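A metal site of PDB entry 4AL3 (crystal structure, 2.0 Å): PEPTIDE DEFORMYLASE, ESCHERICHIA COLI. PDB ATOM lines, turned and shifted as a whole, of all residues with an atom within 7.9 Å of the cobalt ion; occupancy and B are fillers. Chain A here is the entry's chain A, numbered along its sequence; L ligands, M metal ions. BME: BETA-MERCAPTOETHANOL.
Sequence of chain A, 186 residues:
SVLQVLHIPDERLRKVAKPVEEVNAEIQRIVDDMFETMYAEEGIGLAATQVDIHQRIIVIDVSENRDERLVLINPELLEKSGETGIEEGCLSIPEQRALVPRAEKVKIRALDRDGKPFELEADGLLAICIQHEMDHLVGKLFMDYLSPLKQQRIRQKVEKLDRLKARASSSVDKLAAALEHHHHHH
Residues that only touch the cobalt ion: Gln 50 (3.6 Å). The nearest printed residue that does not touch the cobalt ion is Glu 133 (4.1 Å).
A ring nitrogen (NE2) of His 136 lies close to the side-chain amide nitrogen (NE2) of Gln 50 (3.4 Å). SG of CSO 90 lies close to the backbone NH of Ser 92. SG of CSO 90 sits close to the side-chain amide nitrogen (NE2) of Gln 50, at 3.7 Å. ND1 of His 132 is in hydrogen-bond range of OE1 of Glu 88 (2.8 Å). The backbone NH of Ala 47 is in hydrogen-bond range of the side-chain amide oxygen of Gln 50, at 3.1 Å. OE1 of Glu 133 lies close to OE1 of Gln 50 (3.4 Å). The side-chain hydroxyl (OG) of Ser 92 lies within hydrogen-bond range of the side-chain amide nitrogen (NE2) of Gln 50 (2.9 Å).
The cobalt ion is bound by a ring nitrogen (NE2) of His 132 (2.1 Å), SG of CSO 90 (2.2 Å), a sulfur (S2) of the ligand (2.2 Å) and a ring nitrogen (NE2) of His 136 (2.3 Å).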
ATOM      1  N   LEU A  13     -18.043 -12.116   4.308  1.00  0.00           N
ATOM      2  CA  LEU A  13     -17.144 -13.135   4.912  1.00  0.00           C
ATOM      3  C   LEU A  13     -17.874 -14.353   5.562  1.00  0.00           C
ATOM      4  O   LEU A  13     -17.242 -15.392   5.866  1.00  0.00           O
ATOM      5  CB  LEU A  13     -16.224 -12.483   5.971  1.00  0.00           C
ATOM      6  CG  LEU A  13     -15.053 -11.596   5.517  1.00  0.00           C
ATOM      7  CD1 LEU A  13     -14.386 -10.987   6.753  1.00  0.00           C
ATOM      8  CD2 LEU A  13     -14.048 -12.381   4.688  1.00  0.00           C
ATOM      9  N   GLY A  45      -2.033 -18.433   3.128  1.00  0.00           N
ATOM     10  CA  GLY A  45      -3.281 -18.923   2.551  1.00  0.00           C
ATOM     11  C   GLY A  45      -4.278 -17.815   2.198  1.00  0.00           C
ATOM     12  O   GLY A  45      -4.158 -16.674   2.667  1.00  0.00           O
ATOM     13  N   LEU A  46      -5.266 -18.158   1.369  1.00  0.00           N
ATOM     14  CA  LEU A  46      -6.345 -17.229   0.968  1.00  0.00           C
ATOM     15  C   LEU A  46      -7.519 -18.041   0.367  1.00  0.00           C
ATOM     16  O   LEU A  46      -7.329 -18.848  -0.529  1.00  0.00           O
ATOM     17  CB  LEU A  46      -5.841 -16.194  -0.067  1.00  0.00           C
ATOM     18  CG  LEU A  46      -6.876 -15.124  -0.475  1.00  0.00           C
ATOM     19  CD1 LEU A  46      -7.094 -14.142   0.665  1.00  0.00           C
ATOM     20  CD2 LEU A  46      -6.490 -14.396  -1.770  1.00  0.00           C
ATOM     21  N   ALA A  47      -8.716 -17.832   0.907  1.00  0.00           N
ATOM     22  CA  ALA A  47      -9.935 -18.450   0.379  1.00  0.00           C
ATOM     23  C   ALA A  47     -10.625 -17.415  -0.506  1.00  0.00           C
ATOM     24  O   ALA A  47     -10.531 -16.226  -0.257  1.00  0.00           O
ATOM     25  CB  ALA A  47     -10.856 -18.896   1.511  1.00  0.00           C
ATOM     26  N   GLN A  50     -12.825 -14.594   0.932  1.00  0.00           N
ATOM     27  CA  GLN A  50     -12.147 -13.413   1.469  1.00  0.00           C
ATOM     28  C   GLN A  50     -11.967 -12.231   0.482  1.00  0.00           C
ATOM     29  O   GLN A  50     -11.752 -11.121   0.930  1.00  0.00           O
ATOM     30  CB  GLN A  50     -10.758 -13.811   1.989  1.00  0.00           C
ATOM     31  CG  GLN A  50     -10.781 -14.618   3.283  1.00  0.00           C
ATOM     32  CD  GLN A  50      -9.387 -14.913   3.757  1.00  0.00           C
ATOM     33  OE1 GLN A  50      -8.711 -15.810   3.231  1.00  0.00           O
ATOM     34  NE2 GLN A  50      -8.927 -14.139   4.747  1.00  0.00           N
ATOM     35  N   GLU A  88      -2.867 -18.510  15.628  1.00  0.00           N
ATOM     36  CA  GLU A  88      -3.202 -18.253  14.217  1.00  0.00           C
ATOM     37  C   GLU A  88      -3.523 -16.754  13.937  1.00  0.00           C
ATOM     38  O   GLU A  88      -4.062 -16.068  14.787  1.00  0.00           O
ATOM     39  CB  GLU A  88      -4.420 -19.097  13.788  1.00  0.00           C
ATOM     40  CG  GLU A  88      -4.190 -20.621  13.677  1.00  0.00           C
ATOM     41  CD  GLU A  88      -5.444 -21.358  13.156  1.00  0.00           C
ATOM     42  OE1 GLU A  88      -6.274 -20.762  12.417  1.00  0.00           O
ATOM     43  OE2 GLU A  88      -5.631 -22.554  13.510  1.00  0.00           O
ATOM     44  N   GLY A  89      -3.209 -16.307  12.705  1.00  0.00           N
ATOM     45  CA  GLY A  89      -3.635 -15.008  12.177  1.00  0.00           C
ATOM     46  C   GLY A  89      -4.563 -15.171  10.982  1.00  0.00           C
ATOM     47  O   GLY A  89      -4.851 -16.285  10.557  1.00  0.00           O
ATOM     48  N   CSO A  90      -5.014 -14.031  10.447  1.00  0.00           N
ATOM     49  CA  CSO A  90      -6.002 -14.013   9.367  1.00  0.00           C
ATOM     50  CB  CSO A  90      -7.424 -14.278   9.840  1.00  0.00           C
ATOM     51  SG  CSO A  90      -8.409 -14.632   8.422  1.00  0.00           S
ATOM     52  C   CSO A  90      -5.944 -12.676   8.666  1.00  0.00           C
ATOM     53  O   CSO A  90      -5.969 -11.608   9.306  1.00  0.00           O
ATOM     54  OD  CSO A  90     -10.063 -14.248   8.739  1.00  0.00           O
ATOM     55  N   LEU A  91      -5.887 -12.739   7.334  1.00  0.00           N
ATOM     56  CA  LEU A  91      -5.819 -11.541   6.516  1.00  0.00           C
ATOM     57  C   LEU A  91      -7.118 -10.694   6.663  1.00  0.00           C
ATOM     58  O   LEU A  91      -7.092  -9.462   6.503  1.00  0.00           O
ATOM     59  CB  LEU A  91      -5.474 -11.890   5.029  1.00  0.00           C
ATOM     60  CG  LEU A  91      -4.177 -12.705   4.748  1.00  0.00           C
ATOM     61  CD1 LEU A  91      -3.889 -12.882   3.255  1.00  0.00           C
ATOM     62  CD2 LEU A  91      -2.946 -12.107   5.427  1.00  0.00           C
ATOM     63  N   SER A  92      -8.240 -11.345   7.014  1.00  0.00           N
ATOM     64  CA  SER A  92      -9.524 -10.649   7.250  1.00  0.00           C
ATOM     65  C   SER A  92      -9.732 -10.180   8.723  1.00  0.00           C
ATOM     66  O   SER A  92     -10.768  -9.599   9.046  1.00  0.00           O
ATOM     67  CB  SER A  92     -10.690 -11.512   6.768  1.00  0.00           C
ATOM     68  OG  SER A  92     -10.525 -11.849   5.401  1.00  0.00           O
ATOM     69  N   ILE A  93      -8.748 -10.441   9.583  1.00  0.00           N
ATOM     70  CA  ILE A  93      -8.763 -10.044  10.999  1.00  0.00           C
ATOM     71  C   ILE A  93      -7.368  -9.489  11.313  1.00  0.00           C
ATOM     72  O   ILE A  93      -6.602 -10.119  12.045  1.00  0.00           O
ATOM     73  CB  ILE A  93      -9.094 -11.226  11.966  1.00  0.00           C
ATOM     74  CG1 ILE A  93     -10.248 -12.086  11.421  1.00  0.00           C
ATOM     75  CG2 ILE A  93      -9.406 -10.716  13.375  1.00  0.00           C
ATOM     76  CD1 ILE A  93     -10.657 -13.221  12.341  1.00  0.00           C
ATOM     77  N   ARG A 102      -7.246 -27.594  16.466  1.00  0.00           N
ATOM     78  CA  ARG A 102      -7.204 -28.109  15.099  1.00  0.00           C
ATOM     79  C   ARG A 102      -6.856 -29.589  15.119  1.00  0.00           C
ATOM     80  O   ARG A 102      -6.198 -30.060  16.046  1.00  0.00           O
ATOM     81  CB  ARG A 102      -6.116 -27.377  14.293  1.00  0.00           C
ATOM     82  CG  ARG A 102      -6.388 -25.908  14.016  1.00  0.00           C
ATOM     83  CD  ARG A 102      -7.575 -25.688  13.082  1.00  0.00           C
ATOM     84  NE  ARG A 102      -7.723 -24.275  12.750  1.00  0.00           N
ATOM     85  CZ  ARG A 102      -8.775 -23.695  12.185  1.00  0.00           C
ATOM     86  NH1 ARG A 102      -9.844 -24.418  11.835  1.00  0.00           N
ATOM     87  NH2 ARG A 102      -8.761 -22.373  11.955  1.00  0.00           N
ATOM     88  N   CYS A 129      -3.243 -24.725   8.245  1.00  0.00           N
ATOM     89  CA  CYS A 129      -3.624 -23.778   7.185  1.00  0.00           C
ATOM     90  C   CYS A 129      -4.760 -24.324   6.275  1.00  0.00           C
ATOM     91  O   CYS A 129      -5.682 -23.588   5.930  1.00  0.00           O
ATOM     92  CB  CYS A 129      -2.399 -23.386   6.345  1.00  0.00           C
ATOM     93  SG  CYS A 129      -2.776 -22.130   5.102  1.00  0.00           S
ATOM     94  N   HIS A 132      -7.900 -23.925   8.239  1.00  0.00           N
ATOM     95  CA  HIS A 132      -8.222 -22.482   8.348  1.00  0.00           C
ATOM     96  C   HIS A 132      -8.990 -21.989   7.129  1.00  0.00           C
ATOM     97  O   HIS A 132     -10.054 -21.360   7.246  1.00  0.00           O
ATOM     98  CB  HIS A 132      -6.897 -21.695   8.514  1.00  0.00           C
ATOM     99  CG  HIS A 132      -7.071 -20.223   8.756  1.00  0.00           C
ATOM    100  ND1 HIS A 132      -6.889 -19.641   9.980  1.00  0.00           N
ATOM    101  CD2 HIS A 132      -7.393 -19.174   7.867  1.00  0.00           C
ATOM    102  CE1 HIS A 132      -7.061 -18.317   9.878  1.00  0.00           C
ATOM    103  NE2 HIS A 132      -7.398 -18.032   8.595  1.00  0.00           N
ATOM    104  N   GLU A 133      -8.431 -22.279   5.952  1.00  0.00           N
ATOM    105  CA  GLU A 133      -8.951 -21.806   4.675  1.00  0.00           C
ATOM    106  C   GLU A 133     -10.249 -22.513   4.250  1.00  0.00           C
ATOM    107  O   GLU A 133     -11.104 -21.883   3.632  1.00  0.00           O
ATOM    108  CB  GLU A 133      -7.871 -21.899   3.546  1.00  0.00           C
ATOM    109  CG  GLU A 133      -6.592 -21.091   3.773  1.00  0.00           C
ATOM    110  CD  GLU A 133      -6.836 -19.592   3.939  1.00  0.00           C
ATOM    111  OE1 GLU A 133      -7.816 -19.079   3.364  1.00  0.00           O
ATOM    112  OE2 GLU A 133      -6.053 -18.901   4.648  1.00  0.00           O
ATOM    113  N   ASP A 135     -12.465 -23.532   6.375  1.00  0.00           N
ATOM    114  CA  ASP A 135     -13.410 -22.817   7.257  1.00  0.00           C
ATOM    115  C   ASP A 135     -13.996 -21.559   6.579  1.00  0.00           C
ATOM    116  O   ASP A 135     -15.203 -21.326   6.680  1.00  0.00           O
ATOM    117  CB  ASP A 135     -12.771 -22.409   8.612  1.00  0.00           C
ATOM    118  CG  ASP A 135     -12.925 -23.485   9.718  1.00  0.00           C
ATOM    119  OD1 ASP A 135     -13.481 -24.564   9.456  1.00  0.00           O
ATOM    120  OD2 ASP A 135     -12.490 -23.228  10.861  1.00  0.00           O
ATOM    121  N   HIS A 136     -13.140 -20.755   5.941  1.00  0.00           N
ATOM    122  CA  HIS A 136     -13.597 -19.582   5.144  1.00  0.00           C
ATOM    123  C   HIS A 136     -14.670 -19.889   4.132  1.00  0.00           C
ATOM    124  O   HIS A 136     -15.618 -19.110   3.986  1.00  0.00           O
ATOM    125  CB  HIS A 136     -12.444 -18.929   4.362  1.00  0.00           C
ATOM    126  CG  HIS A 136     -11.550 -18.055   5.199  1.00  0.00           C
ATOM    127  ND1 HIS A 136     -11.999 -16.971   5.848  1.00  0.00           N
ATOM    128  CD2 HIS A 136     -10.181 -18.117   5.422  1.00  0.00           C
ATOM    129  CE1 HIS A 136     -10.985 -16.385   6.486  1.00  0.00           C
ATOM    130  NE2 HIS A 136      -9.863 -17.093   6.216  1.00  0.00           N
ATOM    131  N   LYS A 140     -16.617 -19.376   8.085  1.00  0.00           N
ATOM    132  CA  LYS A 140     -16.108 -19.515   9.463  1.00  0.00           C
ATOM    133  C   LYS A 140     -14.712 -18.867   9.645  1.00  0.00           C
ATOM    134  O   LYS A 140     -13.827 -18.972   8.784  1.00  0.00           O
ATOM    135  CB  LYS A 140     -16.118 -21.002   9.873  1.00  0.00           C
ATOM    136  CG  LYS A 140     -15.993 -21.231  11.374  1.00  0.00           C
ATOM    137  CD  LYS A 140     -16.190 -22.704  11.726  1.00  0.00           C
ATOM    138  CE  LYS A 140     -16.201 -22.910  13.245  1.00  0.00           C
ATOM    139  NZ  LYS A 140     -16.065 -24.337  13.668  1.00  0.00           N
ATOM    140  N   LEU A 141     -14.552 -18.176  10.779  1.00  0.00           N
ATOM    141  CA  LEU A 141     -13.317 -17.460  11.148  1.00  0.00           C
ATOM    142  C   LEU A 141     -12.686 -18.083  12.409  1.00  0.00           C
ATOM    143  O   LEU A 141     -13.379 -18.755  13.192  1.00  0.00           O
ATOM    144  CB  LEU A 141     -13.615 -15.962  11.346  1.00  0.00           C
ATOM    145  CG  LEU A 141     -14.168 -15.201  10.117  1.00  0.00           C
ATOM    146  CD1 LEU A 141     -14.749 -13.855  10.507  1.00  0.00           C
ATOM    147  CD2 LEU A 141     -13.123 -15.026   9.015  1.00  0.00           C
ATOM    148  N   PHE A 142     -11.376 -17.881  12.614  1.00  0.00           N
ATOM    149  CA  PHE A 142     -10.683 -18.511  13.759  1.00  0.00           C
ATOM    150  C   PHE A 142     -11.163 -17.973  15.119  1.00  0.00           C
ATOM    151  O   PHE A 142     -11.153 -18.709  16.128  1.00  0.00           O
ATOM    152  CB  PHE A 142      -9.134 -18.419  13.638  1.00  0.00           C
ATOM    153  CG  PHE A 142      -8.563 -17.063  14.002  1.00  0.00           C
ATOM    154  CD1 PHE A 142      -8.428 -16.064  13.041  1.00  0.00           C
ATOM    155  CD2 PHE A 142      -8.148 -16.782  15.314  1.00  0.00           C
ATOM    156  CE1 PHE A 142      -7.887 -14.826  13.356  1.00  0.00           C
ATOM    157  CE2 PHE A 142      -7.634 -15.529  15.648  1.00  0.00           C
ATOM    158  CZ  PHE A 142      -7.500 -14.550  14.666  1.00  0.00           C
HETATM  159  C1  BME L   1      -3.575 -17.022   6.345  1.00  0.00           C
HETATM  160  C2  BME L   1      -4.522 -15.884   6.011  1.00  0.00           C
HETATM  161  O1  BME L   1      -2.448 -16.600   5.555  1.00  0.00           O
HETATM  162  S2  BME L   1      -6.266 -16.257   5.957  1.00  0.00           S
HETATM  163 CO    CO M   1      -7.957 -16.445   7.348  1.00  0.00          CO
